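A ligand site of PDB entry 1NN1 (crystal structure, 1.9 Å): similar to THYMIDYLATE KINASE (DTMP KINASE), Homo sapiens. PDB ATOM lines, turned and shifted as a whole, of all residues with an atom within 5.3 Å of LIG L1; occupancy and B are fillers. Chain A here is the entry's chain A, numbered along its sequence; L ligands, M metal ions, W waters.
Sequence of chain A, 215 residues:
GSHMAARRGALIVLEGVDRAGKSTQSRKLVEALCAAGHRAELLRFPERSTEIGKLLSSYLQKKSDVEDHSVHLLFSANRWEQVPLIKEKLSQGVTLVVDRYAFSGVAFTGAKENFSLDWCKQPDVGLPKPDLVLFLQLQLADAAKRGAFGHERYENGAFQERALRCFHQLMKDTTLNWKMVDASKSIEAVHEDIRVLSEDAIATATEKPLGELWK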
ATOM      1  N   SER A  23      19.850 -26.036 -12.885  1.00  0.00           N
ATOM      2  CA  SER A  23      19.502 -25.700 -11.463  1.00  0.00           C
ATOM      3  C   SER A  23      20.520 -26.299 -10.512  1.00  0.00           C
ATOM      4  O   SER A  23      20.905 -25.657  -9.537  1.00  0.00           O
ATOM      5  CB  SER A  23      18.117 -26.222 -11.147  1.00  0.00           C
ATOM      6  OG  SER A  23      17.172 -25.446 -11.919  1.00  0.00           O
ATOM      7  N   PHE A  45      14.710 -17.725 -13.190  1.00  0.00           N
ATOM      8  CA  PHE A  45      13.578 -17.242 -14.003  1.00  0.00           C
ATOM      9  C   PHE A  45      12.915 -18.460 -14.618  1.00  0.00           C
ATOM     10  O   PHE A  45      13.615 -19.375 -15.078  1.00  0.00           O
ATOM     11  CB  PHE A  45      13.977 -16.171 -15.016  1.00  0.00           C
ATOM     12  CG  PHE A  45      14.355 -14.874 -14.336  1.00  0.00           C
ATOM     13  CD1 PHE A  45      15.706 -14.537 -14.222  1.00  0.00           C
ATOM     14  CD2 PHE A  45      13.388 -14.061 -13.776  1.00  0.00           C
ATOM     15  CE1 PHE A  45      16.068 -13.351 -13.595  1.00  0.00           C
ATOM     16  CE2 PHE A  45      13.752 -12.877 -13.140  1.00  0.00           C
ATOM     17  CZ  PHE A  45      15.117 -12.503 -13.039  1.00  0.00           C
ATOM     18  N   PRO A  46      11.599 -18.535 -14.593  1.00  0.00           N
ATOM     19  CA  PRO A  46      10.756 -17.513 -14.005  1.00  0.00           C
ATOM     20  C   PRO A  46      10.794 -17.532 -12.489  1.00  0.00           C
ATOM     21  O   PRO A  46      11.105 -18.574 -11.888  1.00  0.00           O
ATOM     22  CB  PRO A  46       9.308 -17.916 -14.419  1.00  0.00           C
ATOM     23  CG  PRO A  46       9.432 -19.391 -14.524  1.00  0.00           C
ATOM     24  CD  PRO A  46      10.784 -19.673 -15.096  1.00  0.00           C
ATOM     25  N   ARG A  48       8.614 -17.473  -9.710  1.00  0.00           N
ATOM     26  CA  ARG A  48       7.180 -17.749  -9.509  1.00  0.00           C
ATOM     27  C   ARG A  48       6.519 -17.153  -8.292  1.00  0.00           C
ATOM     28  O   ARG A  48       5.311 -17.356  -8.148  1.00  0.00           O
ATOM     29  CB  ARG A  48       6.925 -19.272  -9.473  1.00  0.00           C
ATOM     30  CG  ARG A  48       7.549 -20.003 -10.639  1.00  0.00           C
ATOM     31  CD  ARG A  48       7.179 -21.501 -10.603  1.00  0.00           C
ATOM     32  NE  ARG A  48       7.915 -22.180 -11.681  1.00  0.00           N
ATOM     33  CZ  ARG A  48       7.337 -23.182 -12.363  1.00  0.00           C
ATOM     34  NH1 ARG A  48       6.110 -23.568 -12.049  1.00  0.00           N
ATOM     35  NH2 ARG A  48       8.012 -23.776 -13.327  1.00  0.00           N
ATOM     36  N   LEU A  60       2.702 -22.844 -16.908  1.00  0.00           N
ATOM     37  CA  LEU A  60       3.615 -23.959 -17.167  1.00  0.00           C
ATOM     38  C   LEU A  60       3.108 -25.305 -16.656  1.00  0.00           C
ATOM     39  O   LEU A  60       3.498 -26.367 -17.171  1.00  0.00           O
ATOM     40  CB  LEU A  60       4.952 -23.598 -16.485  1.00  0.00           C
ATOM     41  CG  LEU A  60       5.727 -22.514 -17.275  1.00  0.00           C
ATOM     42  CD1 LEU A  60       6.933 -22.079 -16.424  1.00  0.00           C
ATOM     43  CD2 LEU A  60       6.102 -23.061 -18.629  1.00  0.00           C
ATOM     44  N   PHE A  75       6.643 -13.357 -19.303  1.00  0.00           N
ATOM     45  CA  PHE A  75       7.966 -13.873 -18.873  1.00  0.00           C
ATOM     46  C   PHE A  75       8.992 -12.749 -18.805  1.00  0.00           C
ATOM     47  O   PHE A  75       9.908 -12.688 -17.988  1.00  0.00           O
ATOM     48  CB  PHE A  75       8.494 -14.910 -19.923  1.00  0.00           C
ATOM     49  CG  PHE A  75       8.023 -16.322 -19.591  1.00  0.00           C
ATOM     50  CD1 PHE A  75       7.092 -16.961 -20.415  1.00  0.00           C
ATOM     51  CD2 PHE A  75       8.552 -16.994 -18.503  1.00  0.00           C
ATOM     52  CE1 PHE A  75       6.735 -18.260 -20.115  1.00  0.00           C
ATOM     53  CE2 PHE A  75       8.175 -18.286 -18.197  1.00  0.00           C
ATOM     54  CZ  PHE A  75       7.226 -18.921 -19.005  1.00  0.00           C
ATOM     55  N   SER A  76       8.904 -11.825 -19.780  1.00  0.00           N
ATOM     56  CA  SER A  76       9.856 -10.688 -19.831  1.00  0.00           C
ATOM     57  C   SER A  76       9.601  -9.729 -18.683  1.00  0.00           C
ATOM     58  O   SER A  76      10.501  -9.298 -17.939  1.00  0.00           O
ATOM     59  CB  SER A  76       9.793  -9.971 -21.198  1.00  0.00           C
ATOM     60  OG  SER A  76      10.641  -8.823 -21.138  1.00  0.00           O
ATOM     61  N   ARG A  79      11.223 -10.662 -15.538  1.00  0.00           N
ATOM     62  CA  ARG A  79      12.608 -10.276 -15.372  1.00  0.00           C
ATOM     63  C   ARG A  79      12.709  -8.799 -15.037  1.00  0.00           C
ATOM     64  O   ARG A  79      13.476  -8.460 -14.133  1.00  0.00           O
ATOM     65  CB  ARG A  79      13.464 -10.553 -16.660  1.00  0.00           C
ATOM     66  CG  ARG A  79      13.739 -12.062 -16.798  1.00  0.00           C
ATOM     67  CD  ARG A  79      14.433 -12.208 -18.160  1.00  0.00           C
ATOM     68  NE  ARG A  79      13.569 -12.202 -19.331  1.00  0.00           N
ATOM     69  CZ  ARG A  79      12.807 -13.235 -19.694  1.00  0.00           C
ATOM     70  NH1 ARG A  79      12.671 -14.358 -18.959  1.00  0.00           N
ATOM     71  NH2 ARG A  79      12.108 -13.216 -20.844  1.00  0.00           N
ATOM     72  N   ASP A  99      19.618 -18.747 -12.889  1.00  0.00           N
ATOM     73  CA  ASP A  99      19.167 -19.991 -13.482  1.00  0.00           C
ATOM     74  C   ASP A  99      18.069 -19.689 -14.509  1.00  0.00           C
ATOM     75  O   ASP A  99      16.927 -19.523 -14.094  1.00  0.00           O
ATOM     76  CB  ASP A  99      18.658 -20.871 -12.332  1.00  0.00           C
ATOM     77  CG  ASP A  99      18.155 -22.246 -12.731  1.00  0.00           C
ATOM     78  OD1 ASP A  99      18.243 -22.622 -13.917  1.00  0.00           O
ATOM     79  OD2 ASP A  99      17.611 -22.987 -11.851  1.00  0.00           O
ATOM     80  N   ARG A 100      18.448 -19.493 -15.749  1.00  0.00           N
ATOM     81  CA  ARG A 100      17.691 -19.074 -16.910  1.00  0.00           C
ATOM     82  C   ARG A 100      17.476 -17.548 -16.941  1.00  0.00           C
ATOM     83  O   ARG A 100      17.333 -16.978 -15.875  1.00  0.00           O
ATOM     84  CB  ARG A 100      16.284 -19.672 -17.105  1.00  0.00           C
ATOM     85  CG  ARG A 100      16.317 -21.210 -17.360  1.00  0.00           C
ATOM     86  CD  ARG A 100      14.824 -21.545 -17.636  1.00  0.00           C
ATOM     87  NE  ARG A 100      14.556 -22.968 -17.779  1.00  0.00           N
ATOM     88  CZ  ARG A 100      14.746 -23.676 -18.898  1.00  0.00           C
ATOM     89  NH1 ARG A 100      15.210 -23.180 -20.041  1.00  0.00           N
ATOM     90  NH2 ARG A 100      14.429 -24.990 -18.901  1.00  0.00           N
ATOM     91  N   TYR A 101      17.450 -16.970 -18.134  1.00  0.00           N
ATOM     92  CA  TYR A 101      17.281 -15.513 -18.239  1.00  0.00           C
ATOM     93  C   TYR A 101      16.542 -15.213 -19.548  1.00  0.00           C
ATOM     94  O   TYR A 101      15.754 -16.029 -20.030  1.00  0.00           O
ATOM     95  CB  TYR A 101      18.647 -14.843 -18.109  1.00  0.00           C
ATOM     96  CG  TYR A 101      18.754 -13.359 -17.794  1.00  0.00           C
ATOM     97  CD1 TYR A 101      18.069 -12.769 -16.723  1.00  0.00           C
ATOM     98  CD2 TYR A 101      19.525 -12.549 -18.615  1.00  0.00           C
ATOM     99  CE1 TYR A 101      18.233 -11.412 -16.460  1.00  0.00           C
ATOM    100  CE2 TYR A 101      19.686 -11.180 -18.359  1.00  0.00           C
ATOM    101  CZ  TYR A 101      19.039 -10.644 -17.280  1.00  0.00           C
ATOM    102  OH  TYR A 101      19.223  -9.310 -16.976  1.00  0.00           O
ATOM    103  N   SER A 104      16.394 -18.061 -22.530  1.00  0.00           N
ATOM    104  CA  SER A 104      15.348 -19.053 -22.455  1.00  0.00           C
ATOM    105  C   SER A 104      14.019 -18.395 -22.936  1.00  0.00           C
ATOM    106  O   SER A 104      13.259 -19.026 -23.655  1.00  0.00           O
ATOM    107  CB  SER A 104      15.076 -19.535 -21.029  1.00  0.00           C
ATOM    108  OG  SER A 104      16.001 -20.592 -20.725  1.00  0.00           O
ATOM    109  N   GLY A 105      13.785 -17.148 -22.569  1.00  0.00           N
ATOM    110  CA  GLY A 105      12.574 -16.425 -23.033  1.00  0.00           C
ATOM    111  C   GLY A 105      12.450 -16.454 -24.546  1.00  0.00           C
ATOM    112  O   GLY A 105      11.371 -16.744 -25.111  1.00  0.00           O
ATOM    113  N   PHE A 108      12.298 -20.368 -26.139  1.00  0.00           N
ATOM    114  CA  PHE A 108      11.050 -21.049 -25.955  1.00  0.00           C
ATOM    115  C   PHE A 108       9.932 -20.427 -26.771  1.00  0.00           C
ATOM    116  O   PHE A 108       9.204 -21.201 -27.403  1.00  0.00           O
ATOM    117  CB  PHE A 108      10.635 -21.246 -24.462  1.00  0.00           C
ATOM    118  CG  PHE A 108      11.459 -22.396 -23.920  1.00  0.00           C
ATOM    119  CD1 PHE A 108      12.835 -22.251 -23.796  1.00  0.00           C
ATOM    120  CD2 PHE A 108      10.858 -23.597 -23.611  1.00  0.00           C
ATOM    121  CE1 PHE A 108      13.611 -23.318 -23.357  1.00  0.00           C
ATOM    122  CE2 PHE A 108      11.647 -24.660 -23.152  1.00  0.00           C
ATOM    123  CZ  PHE A 108      13.018 -24.533 -23.065  1.00  0.00           C
ATOM    124  N   THR A 109       9.731 -19.100 -26.739  1.00  0.00           N
ATOM    125  CA  THR A 109       8.632 -18.578 -27.568  1.00  0.00           C
ATOM    126  C   THR A 109       9.043 -18.738 -29.034  1.00  0.00           C
ATOM    127  O   THR A 109       8.257 -19.004 -29.944  1.00  0.00           O
ATOM    128  CB  THR A 109       8.388 -17.087 -27.208  1.00  0.00           C
ATOM    129  OG1 THR A 109       7.912 -17.046 -25.841  1.00  0.00           O
ATOM    130  CG2 THR A 109       7.359 -16.461 -28.149  1.00  0.00           C
ATOM    131  N   GLU A 152       5.079 -30.550 -17.306  1.00  0.00           N
ATOM    132  CA  GLU A 152       4.868 -29.133 -17.618  1.00  0.00           C
ATOM    133  C   GLU A 152       4.879 -28.940 -19.143  1.00  0.00           C
ATOM    134  O   GLU A 152       5.295 -29.764 -19.931  1.00  0.00           O
ATOM    135  CB  GLU A 152       5.887 -28.210 -16.970  1.00  0.00           C
ATOM    136  CG  GLU A 152       5.790 -27.978 -15.474  1.00  0.00           C
ATOM    137  CD  GLU A 152       6.471 -26.726 -14.959  1.00  0.00           C
ATOM    138  OE1 GLU A 152       5.942 -26.178 -13.957  1.00  0.00           O
ATOM    139  OE2 GLU A 152       7.504 -26.245 -15.502  1.00  0.00           O
ATOM    140  N   TYR A 154       5.987 -27.607 -22.826  1.00  0.00           N
ATOM    141  CA  TYR A 154       7.274 -27.651 -23.492  1.00  0.00           C
ATOM    142  C   TYR A 154       8.119 -28.901 -23.189  1.00  0.00           C
ATOM    143  O   TYR A 154       9.202 -28.994 -23.773  1.00  0.00           O
ATOM    144  CB  TYR A 154       8.115 -26.415 -23.124  1.00  0.00           C
ATOM    145  CG  TYR A 154       7.430 -25.069 -23.271  1.00  0.00           C
ATOM    146  CD1 TYR A 154       7.707 -24.010 -22.399  1.00  0.00           C
ATOM    147  CD2 TYR A 154       6.489 -24.840 -24.270  1.00  0.00           C
ATOM    148  CE1 TYR A 154       7.108 -22.785 -22.548  1.00  0.00           C
ATOM    149  CE2 TYR A 154       5.867 -23.614 -24.425  1.00  0.00           C
ATOM    150  CZ  TYR A 154       6.166 -22.591 -23.568  1.00  0.00           C
ATOM    151  OH  TYR A 154       5.566 -21.356 -23.714  1.00  0.00           O
HETATM  152  P1  LIG L   1      11.882 -24.504 -14.753  1.00  0.00           P
HETATM  153  O1  LIG L   1      11.018 -23.640 -13.814  1.00  0.00           O
HETATM  154  O2  LIG L   1      11.569 -25.897 -14.385  1.00  0.00           O
HETATM  155  O3  LIG L   1      13.249 -23.856 -14.973  1.00  0.00           O
HETATM  156  O4  LIG L   1      11.025 -24.380 -16.092  1.00  0.00           O
HETATM  157  N1  LIG L   1      10.697 -20.310 -20.061  1.00  0.00           N
HETATM  158  C1  LIG L   1      11.527 -19.765 -19.127  1.00  0.00           C
HETATM  159  C2  LIG L   1       9.957 -19.564 -21.026  1.00  0.00           C
HETATM  160  O5  LIG L   1       9.199 -20.182 -21.785  1.00  0.00           O
HETATM  161  N2  LIG L   1      10.261 -18.223 -21.077  1.00  0.00           N
HETATM  162  C3  LIG L   1      11.142 -17.628 -20.160  1.00  0.00           C
HETATM  163  O6  LIG L   1      11.352 -16.278 -20.220  1.00  0.00           O
HETATM  164  C4  LIG L   1      11.805 -18.424 -19.151  1.00  0.00           C
HETATM  165  C5  LIG L   1      12.767 -17.737 -18.179  1.00  0.00           C
HETATM  166  C6  LIG L   1      11.552 -22.600 -19.927  1.00  0.00           C
HETATM  167  C7  LIG L   1      10.660 -23.204 -16.789  1.00  0.00           C
HETATM  168  C8  LIG L   1      10.052 -23.306 -18.199  1.00  0.00           C
HETATM  169  O7  LIG L   1       9.724 -21.970 -18.703  1.00  0.00           O
HETATM  170  C9  LIG L   1      10.318 -21.695 -19.890  1.00  0.00           C
HETATM  171  C10 LIG L   1      11.051 -23.849 -19.259  1.00  0.00           C
HETATM  172  P1  LG2 L   2      15.037 -28.061 -16.198  1.00  0.00           P
HETATM  173  O1  LG2 L   2      14.000 -29.138 -16.184  1.00  0.00           O
HETATM  174  O2  LG2 L   2      14.817 -27.028 -15.205  1.00  0.00           O
HETATM  175  O3  LG2 L   2      15.517 -27.589 -17.555  1.00  0.00           O
HETATM  176  P2  LG2 L   2      17.786 -28.479 -15.166  1.00  0.00           P
HETATM  177  O4  LG2 L   2      18.600 -28.200 -16.324  1.00  0.00           O
HETATM  178  O5  LG2 L   2      17.629 -27.372 -14.228  1.00  0.00           O
HETATM  179  N1  LG2 L   2      16.307 -29.032 -15.738  1.00  0.00           N
HETATM  180  P3  LG2 L   2      18.616 -30.187 -13.014  1.00  0.00           P
HETATM  181  O6  LG2 L   2      19.795 -29.538 -12.401  1.00  0.00           O
HETATM  182  O7  LG2 L   2      17.333 -30.079 -12.286  1.00  0.00           O
HETATM  183  O8  LG2 L   2      18.498 -29.767 -14.547  1.00  0.00           O
HETATM  184  O9  LG2 L   2      18.935 -31.767 -13.183  1.00  0.00           O
HETATM  185  C1  LG2 L   2      17.992 -32.653 -13.836  1.00  0.00           C
HETATM  186  C2  LG2 L   2      18.146 -34.079 -13.280  1.00  0.00           C
HETATM  187  O10 LG2 L   2      19.368 -34.599 -13.760  1.00  0.00           O
HETATM  188  C3  LG2 L   2      18.257 -34.080 -11.741  1.00  0.00           C
HETATM  189  O11 LG2 L   2      17.788 -35.306 -11.105  1.00  0.00           O
HETATM  190  C4  LG2 L   2      19.732 -33.990 -11.496  1.00  0.00           C
HETATM  191  O12 LG2 L   2      20.154 -34.620 -10.233  1.00  0.00           O
HETATM  192  C5  LG2 L   2      20.282 -34.796 -12.670  1.00  0.00           C
HETATM  193  N2  LG2 L   2      21.613 -34.283 -13.064  1.00  0.00           N
HETATM  194  C6  LG2 L   2      22.090 -32.988 -13.038  1.00  0.00           C
HETATM  195  N3  LG2 L   2      23.293 -32.873 -13.496  1.00  0.00           N
HETATM  196  C7  LG2 L   2      23.645 -34.173 -13.809  1.00  0.00           C
HETATM  197  C8  LG2 L   2      24.864 -34.670 -14.356  1.00  0.00           C
HETATM  198  N4  LG2 L   2      25.930 -33.861 -14.610  1.00  0.00           N
HETATM  199  N5  LG2 L   2      24.883 -35.989 -14.540  1.00  0.00           N
HETATM  200  C9  LG2 L   2      23.815 -36.735 -14.255  1.00  0.00           C
HETATM  201  N6  LG2 L   2      22.631 -36.371 -13.778  1.00  0.00           N
HETATM  202  C10 LG2 L   2      22.645 -35.029 -13.563  1.00  0.00           C
HETATM  203 MG    MG M   1      15.986 -26.396 -13.514  1.00  0.00          MG
HETATM  204  O   HOH W   1       9.258 -16.588 -23.098  1.00  0.00           O
HETATM  205  O   HOH W   2      14.790 -21.490 -13.780  1.00  0.00           O
HETATM  206  O   HOH W   3      12.755 -27.973 -13.688  1.00  0.00           O
HETATM  207  O   HOH W   4       7.479 -19.301 -23.791  1.00  0.00           O
HETATM  208  O   HOH W   5      10.623 -25.399 -11.114  1.00  0.00           O
HETATM  209  O   HOH W   6      16.455 -24.498 -14.624  1.00  0.00           O
HETATM  210  O   HOH W   7       8.617 -26.271 -18.960  1.00  0.00           O
HETATM  211  O   HOH W   8      14.237 -25.374 -12.731  1.00  0.00           O
HETATM  212  O   HOH W   9      11.732 -21.198 -12.162  1.00  0.00           O
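The backbone NH of Phe 45 sits at hydrogen-bond distance from the backbone carbonyl oxygen of Asp 99 (3.0 Å). The guanidinium group of Arg 48 is in salt-bridge range of the side-chain carboxylate of Glu 152, 3.2 Å away. The side-chain hydroxyl (OG) of Ser 104 is in hydrogen-bond range of the guanidinium group (NH1) of Arg 100, 2.8 Å away. The guanidinium group (NH1) of Arg 79 is in hydrogen-bond range of the backbone carbonyl oxygen (O) of Phe 75 (3.4 Å).
NH2 of Arg 100 is in salt-bridge range of O3 of LG2 L2. O3 of LIG L1 lies within salt-bridge range of NE of Arg 100, at 3.2 Å. NH2 of Arg 48 lies within salt-bridge range of O1 of LIG L1, 3.0 Å away. N of Ser 23 sits close to O5 of LG2 L2, at 2.9 Å. The backbone NH of Gly 105 lies close to an oxygen (O6) of LIG L1. NH1 of Arg 79 lies within hydrogen-bond range of O6 of LIG L1 (2.6 Å).
Water W3 lies within hydrogen-bond range of an oxygen (O2) of LIG L1 and an oxygen (O1) of LG2 L2. Water W1 lies within hydrogen-bond range of a nitrogen (N2) of LIG L1 (2.8 Å), the backbone carbonyl oxygen of Gly 105 (2.9 Å) and the side-chain hydroxyl of Thr 109 (3.1 Å). Water W4 lies within hydrogen-bond range of O5 of LIG L1 (2.8 Å), OH of Tyr 154 (2.8 Å) and OG1 of Thr 109 (3.1 Å). Water W9 bridges the backbone carbonyl oxygen (O) of Pro 46 and an oxygen (O1) of LIG L1. Water W2 lies within hydrogen-bond range of O of Phe 45 (2.7 Å), O of Asp 99 (2.9 Å) and O3 of LIG L1 (3.1 Å). Water W6 bridges OD1 of Asp 99 (2.7 Å) and O3 of LIG L1 (3.3 Å).
Phe 45 touches LIG L1 (O to C5, 3.6 Å). N of Pro 46 touches C5 of LIG L1, at 3.9 Å. Leu 60 touches LIG L1. Phe 75 touches LIG L1. O of Tyr 101 touches C5 of LIG L1, 3.9 Å away. Ser 104 touches LIG L1 (CB to C4, 3.9 Å). Phe 108 touches LIG L1. CE1 of Tyr 154 touches O5 of LIG L1, at 3.4 Å. Hydrophobic or aromatic side chains that line LIG L1: Phe 45, Pro 46, Leu 60, Phe 75, Phe 108 and Tyr 154. Within 4 Å of LIG L1: Phe 45, Pro 46, Arg 48, Leu 60, Phe 75, Arg 79, Arg 100, Tyr 101, Ser 104, Gly 105, Phe 108 and Tyr 154. Along chain A the residues within 4 Å of LIG L1 span positions 45 to 154. The nearest printed residue that does not touch LIG L1 is Glu 152 (4.03 Å).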
